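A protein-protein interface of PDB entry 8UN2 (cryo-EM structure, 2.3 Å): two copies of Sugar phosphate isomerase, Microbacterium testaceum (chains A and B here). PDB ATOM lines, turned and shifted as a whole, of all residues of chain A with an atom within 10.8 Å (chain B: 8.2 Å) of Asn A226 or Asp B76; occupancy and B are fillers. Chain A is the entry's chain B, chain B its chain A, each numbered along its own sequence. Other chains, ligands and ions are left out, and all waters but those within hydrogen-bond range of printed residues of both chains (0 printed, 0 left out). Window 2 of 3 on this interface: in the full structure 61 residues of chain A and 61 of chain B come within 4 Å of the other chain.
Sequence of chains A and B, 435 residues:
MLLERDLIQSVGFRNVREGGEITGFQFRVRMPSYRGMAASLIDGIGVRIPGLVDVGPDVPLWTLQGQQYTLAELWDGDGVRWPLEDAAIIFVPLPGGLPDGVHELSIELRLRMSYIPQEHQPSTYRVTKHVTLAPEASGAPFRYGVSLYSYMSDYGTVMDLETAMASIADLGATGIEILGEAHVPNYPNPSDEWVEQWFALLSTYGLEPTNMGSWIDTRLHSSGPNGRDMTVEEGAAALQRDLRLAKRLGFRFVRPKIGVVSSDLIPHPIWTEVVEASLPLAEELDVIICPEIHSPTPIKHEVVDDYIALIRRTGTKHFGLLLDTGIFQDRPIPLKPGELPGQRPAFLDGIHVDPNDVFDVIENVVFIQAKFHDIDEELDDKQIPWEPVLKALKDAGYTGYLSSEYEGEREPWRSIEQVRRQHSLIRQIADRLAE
O of His A221 is in hydrogen-bond range of N of Arg A228 (2.7 Å).
Of the 13 printed residues of chain B, 5 touch a printed residue of chain A. Printed residues of chain B that touch a printed residue of chain A: Ser B40, Trp B75, Asp B76, Gly B77 and Asp B78. Hydrophobic or aromatic side chains of chain B that line the printed part of chain A: Trp B75. Among the printed residues, 7 pairs touch across the chains. Among the printed residues, no Asp or Glu carboxylate lies within 4 Å of a Lys or Arg side-chain nitrogen of the other chain.
Printed residues of chain B within 4 Å of Leu A220: Ser B40. Of the printed residues of chain B, His A221 touches Trp B75, Gly B77 and Asp B78. Of the printed residues of chain B, Ser A223 touches Trp B75. No residue of chain B comes within 4 Å of Pro A225. No residue of chain B comes within 4 Å of Gly A227. Printed residues of chain A within 4 Å of Ser B40: Leu A220 (2.7 Å). Ala B72 touches none of the printed residues of chain A. Printed residues of chain A within 4 Å of Trp B75: His A221 (3.3 Å), Ser A223 (3.6 Å) and Gly A224 (3.6 Å). Of chain A, only Asn A226 (3.3 Å) comes within 4 Å of Asp B76. The nearest residue of chain A that does not touch Asp B76 is His A221 (4.5 Å). The nearest printed residue of chain A that does not touch Trp B75 is Pro A225 (4.9 Å).
OG of Ser B40 lies within hydrogen-bond range of O of Leu A220 (2.7 Å). The backbone carbonyl oxygen of Trp B75 is in hydrogen-bond range of a ring nitrogen (ND1) of His A221 (3.3 Å). OD2 of Asp B76 lies within hydrogen-bond range of ND2 of Asn A226, at 3.3 Å. A ring nitrogen (NE2) of His A221 is in hydrogen-bond range of the side-chain carboxylate (OD1) of Asp B78.
CE1 of His A221 touches O of Gly B77 (3.1 Å). Ser A223 touches Trp B75. Gly A224 touches Trp B75.
No position is printed for both chains. Of the 7 pairs that touch across the chains among the printed residues, none has its exchanged pair printed and touching as well.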
ATOM      1  N   THR A 218       9.833  -3.669 -33.017  1.00  0.00           N
ATOM      2  CA  THR A 218      11.002  -3.590 -32.157  1.00  0.00           C
ATOM      3  C   THR A 218      10.651  -3.252 -30.720  1.00  0.00           C
ATOM      4  O   THR A 218      11.455  -3.515 -29.824  1.00  0.00           O
ATOM      5  CB  THR A 218      11.990  -2.566 -32.700  1.00  0.00           C
ATOM      6  OG1 THR A 218      11.388  -1.270 -32.691  1.00  0.00           O
ATOM      7  CG2 THR A 218      12.375  -2.923 -34.108  1.00  0.00           C
ATOM      8  N   ARG A 219       9.474  -2.689 -30.473  1.00  0.00           N
ATOM      9  CA  ARG A 219       9.003  -2.416 -29.125  1.00  0.00           C
ATOM     10  C   ARG A 219       8.048  -3.492 -28.643  1.00  0.00           C
ATOM     11  O   ARG A 219       7.060  -3.194 -27.972  1.00  0.00           O
ATOM     12  CB  ARG A 219       8.344  -1.044 -29.052  1.00  0.00           C
ATOM     13  CG  ARG A 219       9.291   0.092 -29.320  1.00  0.00           C
ATOM     14  CD  ARG A 219       8.563   1.402 -29.359  1.00  0.00           C
ATOM     15  NE  ARG A 219       9.227   2.350 -30.239  1.00  0.00           N
ATOM     16  CZ  ARG A 219       8.605   3.337 -30.864  1.00  0.00           C
ATOM     17  NH1 ARG A 219       7.305   3.505 -30.702  1.00  0.00           N
ATOM     18  NH2 ARG A 219       9.282   4.154 -31.650  1.00  0.00           N
ATOM     19  N   LEU A 220       8.326  -4.743 -29.009  1.00  0.00           N
ATOM     20  CA  LEU A 220       7.446  -5.852 -28.667  1.00  0.00           C
ATOM     21  C   LEU A 220       7.435  -6.111 -27.171  1.00  0.00           C
ATOM     22  O   LEU A 220       6.384  -6.395 -26.593  1.00  0.00           O
ATOM     23  CB  LEU A 220       7.888  -7.100 -29.422  1.00  0.00           C
ATOM     24  CG  LEU A 220       7.018  -8.343 -29.309  1.00  0.00           C
ATOM     25  CD1 LEU A 220       5.794  -8.189 -30.158  1.00  0.00           C
ATOM     26  CD2 LEU A 220       7.806  -9.557 -29.732  1.00  0.00           C
ATOM     27  N   HIS A 221       8.592  -6.006 -26.522  1.00  0.00           N
ATOM     28  CA  HIS A 221       8.702  -6.213 -25.085  1.00  0.00           C
ATOM     29  C   HIS A 221       9.308  -5.004 -24.392  1.00  0.00           C
ATOM     30  O   HIS A 221      10.176  -5.147 -23.534  1.00  0.00           O
ATOM     31  CB  HIS A 221       9.515  -7.465 -24.791  1.00  0.00           C
ATOM     32  CG  HIS A 221       8.857  -8.720 -25.261  1.00  0.00           C
ATOM     33  ND1 HIS A 221       7.774  -9.274 -24.617  1.00  0.00           N
ATOM     34  CD2 HIS A 221       9.113  -9.517 -26.323  1.00  0.00           C
ATOM     35  CE1 HIS A 221       7.398 -10.365 -25.256  1.00  0.00           C
ATOM     36  NE2 HIS A 221       8.194 -10.536 -26.293  1.00  0.00           N
ATOM     37  N   SER A 222       8.853  -3.811 -24.753  1.00  0.00           N
ATOM     38  CA  SER A 222       9.428  -2.594 -24.212  1.00  0.00           C
ATOM     39  C   SER A 222       8.814  -2.207 -22.877  1.00  0.00           C
ATOM     40  O   SER A 222       9.458  -1.512 -22.086  1.00  0.00           O
ATOM     41  CB  SER A 222       9.253  -1.459 -25.212  1.00  0.00           C
ATOM     42  OG  SER A 222       9.755  -0.249 -24.688  1.00  0.00           O
ATOM     43  N   SER A 223       7.586  -2.633 -22.607  1.00  0.00           N
ATOM     44  CA  SER A 223       6.884  -2.203 -21.411  1.00  0.00           C
ATOM     45  C   SER A 223       7.063  -3.201 -20.278  1.00  0.00           C
ATOM     46  O   SER A 223       7.275  -4.395 -20.495  1.00  0.00           O
ATOM     47  CB  SER A 223       5.396  -2.019 -21.696  1.00  0.00           C
ATOM     48  OG  SER A 223       5.181  -0.971 -22.618  1.00  0.00           O
ATOM     49  N   GLY A 224       6.975  -2.692 -19.057  1.00  0.00           N
ATOM     50  CA  GLY A 224       6.980  -3.531 -17.886  1.00  0.00           C
ATOM     51  C   GLY A 224       8.262  -3.454 -17.091  1.00  0.00           C
ATOM     52  O   GLY A 224       9.178  -2.693 -17.412  1.00  0.00           O
ATOM     53  N   PRO A 225       8.343  -4.243 -16.019  1.00  0.00           N
ATOM     54  CA  PRO A 225       9.590  -4.282 -15.244  1.00  0.00           C
ATOM     55  C   PRO A 225      10.697  -5.020 -15.962  1.00  0.00           C
ATOM     56  O   PRO A 225      11.875  -4.683 -15.804  1.00  0.00           O
ATOM     57  CB  PRO A 225       9.175  -5.001 -13.951  1.00  0.00           C
ATOM     58  CG  PRO A 225       7.680  -5.045 -13.976  1.00  0.00           C
ATOM     59  CD  PRO A 225       7.292  -5.060 -15.405  1.00  0.00           C
ATOM     60  N   ASN A 226      10.345  -6.028 -16.753  1.00  0.00           N
ATOM     61  CA  ASN A 226      11.304  -6.787 -17.535  1.00  0.00           C
ATOM     62  C   ASN A 226      11.400  -6.287 -18.965  1.00  0.00           C
ATOM     63  O   ASN A 226      11.657  -7.081 -19.874  1.00  0.00           O
ATOM     64  CB  ASN A 226      10.936  -8.267 -17.517  1.00  0.00           C
ATOM     65  CG  ASN A 226      10.530  -8.741 -16.145  1.00  0.00           C
ATOM     66  OD1 ASN A 226      11.377  -9.056 -15.312  1.00  0.00           O
ATOM     67  ND2 ASN A 226       9.228  -8.793 -15.898  1.00  0.00           N
ATOM     68  N   GLY A 227      11.179  -4.994 -19.180  1.00  0.00           N
ATOM     69  CA  GLY A 227      11.207  -4.410 -20.504  1.00  0.00           C
ATOM     70  C   GLY A 227      12.575  -4.454 -21.143  1.00  0.00           C
ATOM     71  O   GLY A 227      13.569  -4.058 -20.529  1.00  0.00           O
ATOM     72  N   ARG A 228      12.637  -4.939 -22.376  1.00  0.00           N
ATOM     73  CA  ARG A 228      13.899  -5.135 -23.066  1.00  0.00           C
ATOM     74  C   ARG A 228      13.740  -4.741 -24.522  1.00  0.00           C
ATOM     75  O   ARG A 228      12.648  -4.407 -24.984  1.00  0.00           O
ATOM     76  CB  ARG A 228      14.368  -6.583 -22.965  1.00  0.00           C
ATOM     77  CG  ARG A 228      13.273  -7.571 -23.266  1.00  0.00           C
ATOM     78  CD  ARG A 228      13.744  -8.986 -23.080  1.00  0.00           C
ATOM     79  NE  ARG A 228      12.696  -9.941 -23.409  1.00  0.00           N
ATOM     80  CZ  ARG A 228      12.484 -10.419 -24.629  1.00  0.00           C
ATOM     81  NH1 ARG A 228      13.252 -10.030 -25.638  1.00  0.00           N
ATOM     82  NH2 ARG A 228      11.506 -11.285 -24.839  1.00  0.00           N
ATOM     83  N   ASP A 229      14.847  -4.786 -25.245  1.00  0.00           N
ATOM     84  CA  ASP A 229      14.819  -4.477 -26.660  1.00  0.00           C
ATOM     85  C   ASP A 229      14.881  -5.753 -27.485  1.00  0.00           C
ATOM     86  O   ASP A 229      15.430  -6.770 -27.061  1.00  0.00           O
ATOM     87  CB  ASP A 229      15.974  -3.556 -27.029  1.00  0.00           C
ATOM     88  CG  ASP A 229      15.592  -2.550 -28.075  1.00  0.00           C
ATOM     89  OD1 ASP A 229      14.483  -2.670 -28.632  1.00  0.00           O
ATOM     90  OD2 ASP A 229      16.392  -1.633 -28.339  1.00  0.00           O
ATOM     91  N   MET A 230      14.293  -5.690 -28.675  1.00  0.00           N
ATOM     92  CA  MET A 230      14.301  -6.820 -29.589  1.00  0.00           C
ATOM     93  C   MET A 230      15.697  -7.020 -30.155  1.00  0.00           C
ATOM     94  O   MET A 230      16.352  -6.067 -30.580  1.00  0.00           O
ATOM     95  CB  MET A 230      13.293  -6.596 -30.717  1.00  0.00           C
ATOM     96  CG  MET A 230      13.401  -7.574 -31.869  1.00  0.00           C
ATOM     97  SD  MET A 230      12.153  -7.364 -33.145  1.00  0.00           S
ATOM     98  CE  MET A 230      10.851  -8.406 -32.514  1.00  0.00           C
ATOM     99  N   GLU A 234      15.578 -12.556 -32.583  1.00  0.00           N
ATOM    100  CA  GLU A 234      14.133 -12.418 -32.502  1.00  0.00           C
ATOM    101  C   GLU A 234      13.604 -11.578 -33.650  1.00  0.00           C
ATOM    102  O   GLU A 234      12.430 -11.688 -34.020  1.00  0.00           O
ATOM    103  CB  GLU A 234      13.741 -11.799 -31.166  1.00  0.00           C
ATOM    104  CG  GLU A 234      14.298 -12.531 -29.973  1.00  0.00           C
ATOM    105  CD  GLU A 234      14.579 -11.610 -28.812  1.00  0.00           C
ATOM    106  OE1 GLU A 234      14.340 -10.393 -28.945  1.00  0.00           O
ATOM    107  OE2 GLU A 234      15.042 -12.103 -27.763  1.00  0.00           O
ATOM    108  N   ALA B  39      -0.038  -9.377 -28.413  1.00  0.00           N
ATOM    109  CA  ALA B  39      -0.731  -8.831 -27.257  1.00  0.00           C
ATOM    110  C   ALA B  39       0.196  -8.091 -26.314  1.00  0.00           C
ATOM    111  O   ALA B  39      -0.284  -7.374 -25.437  1.00  0.00           O
ATOM    112  CB  ALA B  39      -1.439  -9.951 -26.519  1.00  0.00           C
ATOM    113  N   SER B  40       1.508  -8.236 -26.470  1.00  0.00           N
ATOM    114  CA  SER B  40       2.431  -7.486 -25.636  1.00  0.00           C
ATOM    115  C   SER B  40       2.553  -6.036 -26.073  1.00  0.00           C
ATOM    116  O   SER B  40       3.113  -5.225 -25.333  1.00  0.00           O
ATOM    117  CB  SER B  40       3.794  -8.163 -25.643  1.00  0.00           C
ATOM    118  OG  SER B  40       4.351  -8.151 -26.937  1.00  0.00           O
ATOM    119  N   THR B  70      -3.852 -10.850 -17.315  1.00  0.00           N
ATOM    120  CA  THR B  70      -3.676  -9.498 -16.826  1.00  0.00           C
ATOM    121  C   THR B  70      -2.755  -8.738 -17.771  1.00  0.00           C
ATOM    122  O   THR B  70      -2.189  -9.301 -18.705  1.00  0.00           O
ATOM    123  CB  THR B  70      -3.100  -9.500 -15.416  1.00  0.00           C
ATOM    124  OG1 THR B  70      -1.697  -9.753 -15.483  1.00  0.00           O
ATOM    125  CG2 THR B  70      -3.742 -10.574 -14.591  1.00  0.00           C
ATOM    126  N   LEU B  71      -2.606  -7.437 -17.527  1.00  0.00           N
ATOM    127  CA  LEU B  71      -1.766  -6.630 -18.402  1.00  0.00           C
ATOM    128  C   LEU B  71      -0.294  -6.949 -18.198  1.00  0.00           C
ATOM    129  O   LEU B  71       0.491  -6.917 -19.151  1.00  0.00           O
ATOM    130  CB  LEU B  71      -2.028  -5.147 -18.172  1.00  0.00           C
ATOM    131  CG  LEU B  71      -1.347  -4.206 -19.162  1.00  0.00           C
ATOM    132  CD1 LEU B  71      -1.870  -4.444 -20.553  1.00  0.00           C
ATOM    133  CD2 LEU B  71      -1.531  -2.771 -18.763  1.00  0.00           C
ATOM    134  N   ALA B  72       0.097  -7.284 -16.969  1.00  0.00           N
ATOM    135  CA  ALA B  72       1.484  -7.652 -16.714  1.00  0.00           C
ATOM    136  C   ALA B  72       1.816  -9.007 -17.319  1.00  0.00           C
ATOM    137  O   ALA B  72       2.952  -9.245 -17.734  1.00  0.00           O
ATOM    138  CB  ALA B  72       1.760  -7.653 -15.216  1.00  0.00           C
ATOM    139  N   GLU B  73       0.836  -9.907 -17.382  1.00  0.00           N
ATOM    140  CA  GLU B  73       1.054 -11.189 -18.041  1.00  0.00           C
ATOM    141  C   GLU B  73       1.137 -11.021 -19.547  1.00  0.00           C
ATOM    142  O   GLU B  73       1.809 -11.802 -20.227  1.00  0.00           O
ATOM    143  CB  GLU B  73      -0.065 -12.160 -17.693  1.00  0.00           C
ATOM    144  CG  GLU B  73       0.009 -12.735 -16.310  1.00  0.00           C
ATOM    145  CD  GLU B  73      -1.190 -13.590 -15.992  1.00  0.00           C
ATOM    146  OE1 GLU B  73      -2.202 -13.485 -16.713  1.00  0.00           O
ATOM    147  OE2 GLU B  73      -1.124 -14.370 -15.021  1.00  0.00           O
ATOM    148  N   LEU B  74       0.436 -10.026 -20.087  1.00  0.00           N
ATOM    149  CA  LEU B  74       0.518  -9.753 -21.514  1.00  0.00           C
ATOM    150  C   LEU B  74       1.876  -9.187 -21.884  1.00  0.00           C
ATOM    151  O   LEU B  74       2.398  -9.473 -22.964  1.00  0.00           O
ATOM    152  CB  LEU B  74      -0.581  -8.781 -21.928  1.00  0.00           C
ATOM    153  CG  LEU B  74      -2.000  -9.312 -22.050  1.00  0.00           C
ATOM    154  CD1 LEU B  74      -2.884  -8.254 -22.643  1.00  0.00           C
ATOM    155  CD2 LEU B  74      -2.019 -10.543 -22.899  1.00  0.00           C
ATOM    156  N   TRP B  75       2.467  -8.392 -20.993  1.00  0.00           N
ATOM    157  CA  TRP B  75       3.730  -7.731 -21.297  1.00  0.00           C
ATOM    158  C   TRP B  75       4.881  -8.723 -21.350  1.00  0.00           C
ATOM    159  O   TRP B  75       5.846  -8.522 -22.093  1.00  0.00           O
ATOM    160  CB  TRP B  75       4.011  -6.654 -20.260  1.00  0.00           C
ATOM    161  CG  TRP B  75       3.292  -5.401 -20.522  1.00  0.00           C
ATOM    162  CD1 TRP B  75       2.679  -5.043 -21.671  1.00  0.00           C
ATOM    163  CD2 TRP B  75       3.104  -4.321 -19.612  1.00  0.00           C
ATOM    164  NE1 TRP B  75       2.117  -3.803 -21.543  1.00  0.00           N
ATOM    165  CE2 TRP B  75       2.366  -3.338 -20.282  1.00  0.00           C
ATOM    166  CE3 TRP B  75       3.487  -4.092 -18.293  1.00  0.00           C
ATOM    167  CZ2 TRP B  75       2.005  -2.145 -19.681  1.00  0.00           C
ATOM    168  CZ3 TRP B  75       3.133  -2.911 -17.702  1.00  0.00           C
ATOM    169  CH2 TRP B  75       2.398  -1.951 -18.391  1.00  0.00           C
ATOM    170  N   ASP B  76       4.799  -9.795 -20.578  1.00  0.00           N
ATOM    171  CA  ASP B  76       5.824 -10.825 -20.584  1.00  0.00           C
ATOM    172  C   ASP B  76       5.473 -12.005 -21.475  1.00  0.00           C
ATOM    173  O   ASP B  76       6.294 -12.912 -21.627  1.00  0.00           O
ATOM    174  CB  ASP B  76       6.074 -11.322 -19.164  1.00  0.00           C
ATOM    175  CG  ASP B  76       6.399 -10.202 -18.211  1.00  0.00           C
ATOM    176  OD1 ASP B  76       6.504  -9.047 -18.666  1.00  0.00           O
ATOM    177  OD2 ASP B  76       6.556 -10.473 -17.005  1.00  0.00           O
ATOM    178  N   GLY B  77       4.286 -12.016 -22.065  1.00  0.00           N
ATOM    179  CA  GLY B  77       3.847 -13.173 -22.810  1.00  0.00           C
ATOM    180  C   GLY B  77       4.464 -13.255 -24.191  1.00  0.00           C
ATOM    181  O   GLY B  77       5.040 -12.304 -24.709  1.00  0.00           O
ATOM    182  N   ASP B  78       4.327 -14.433 -24.791  1.00  0.00           N
ATOM    183  CA  ASP B  78       4.792 -14.697 -26.143  1.00  0.00           C
ATOM    184  C   ASP B  78       3.742 -15.505 -26.880  1.00  0.00           C
ATOM    185  O   ASP B  78       3.115 -16.392 -26.299  1.00  0.00           O
ATOM    186  CB  ASP B  78       6.117 -15.454 -26.134  1.00  0.00           C
ATOM    187  CG  ASP B  78       7.285 -14.572 -25.778  1.00  0.00           C
ATOM    188  OD1 ASP B  78       7.276 -13.392 -26.179  1.00  0.00           O
ATOM    189  OD2 ASP B  78       8.204 -15.046 -25.082  1.00  0.00           O
ATOM    190  N   GLY B  79       3.546 -15.191 -28.154  1.00  0.00           N
ATOM    191  CA  GLY B  79       2.652 -15.953 -28.992  1.00  0.00           C
ATOM    192  C   GLY B  79       1.194 -15.569 -28.923  1.00  0.00           C
ATOM    193  O   GLY B  79       0.439 -15.933 -29.828  1.00  0.00           O
ATOM    194  N   VAL B  80       0.769 -14.856 -27.896  1.00  0.00           N
ATOM    195  CA  VAL B  80      -0.620 -14.433 -27.773  1.00  0.00           C
ATOM    196  C   VAL B  80      -0.832 -13.223 -28.662  1.00  0.00           C
ATOM    197  O   VAL B  80      -0.008 -12.305 -28.688  1.00  0.00           O
ATOM    198  CB  VAL B  80      -0.971 -14.115 -26.312  1.00  0.00           C
ATOM    199  CG1 VAL B  80      -2.468 -14.009 -26.143  1.00  0.00           C
ATOM    200  CG2 VAL B  80      -0.408 -15.171 -25.402  1.00  0.00           C
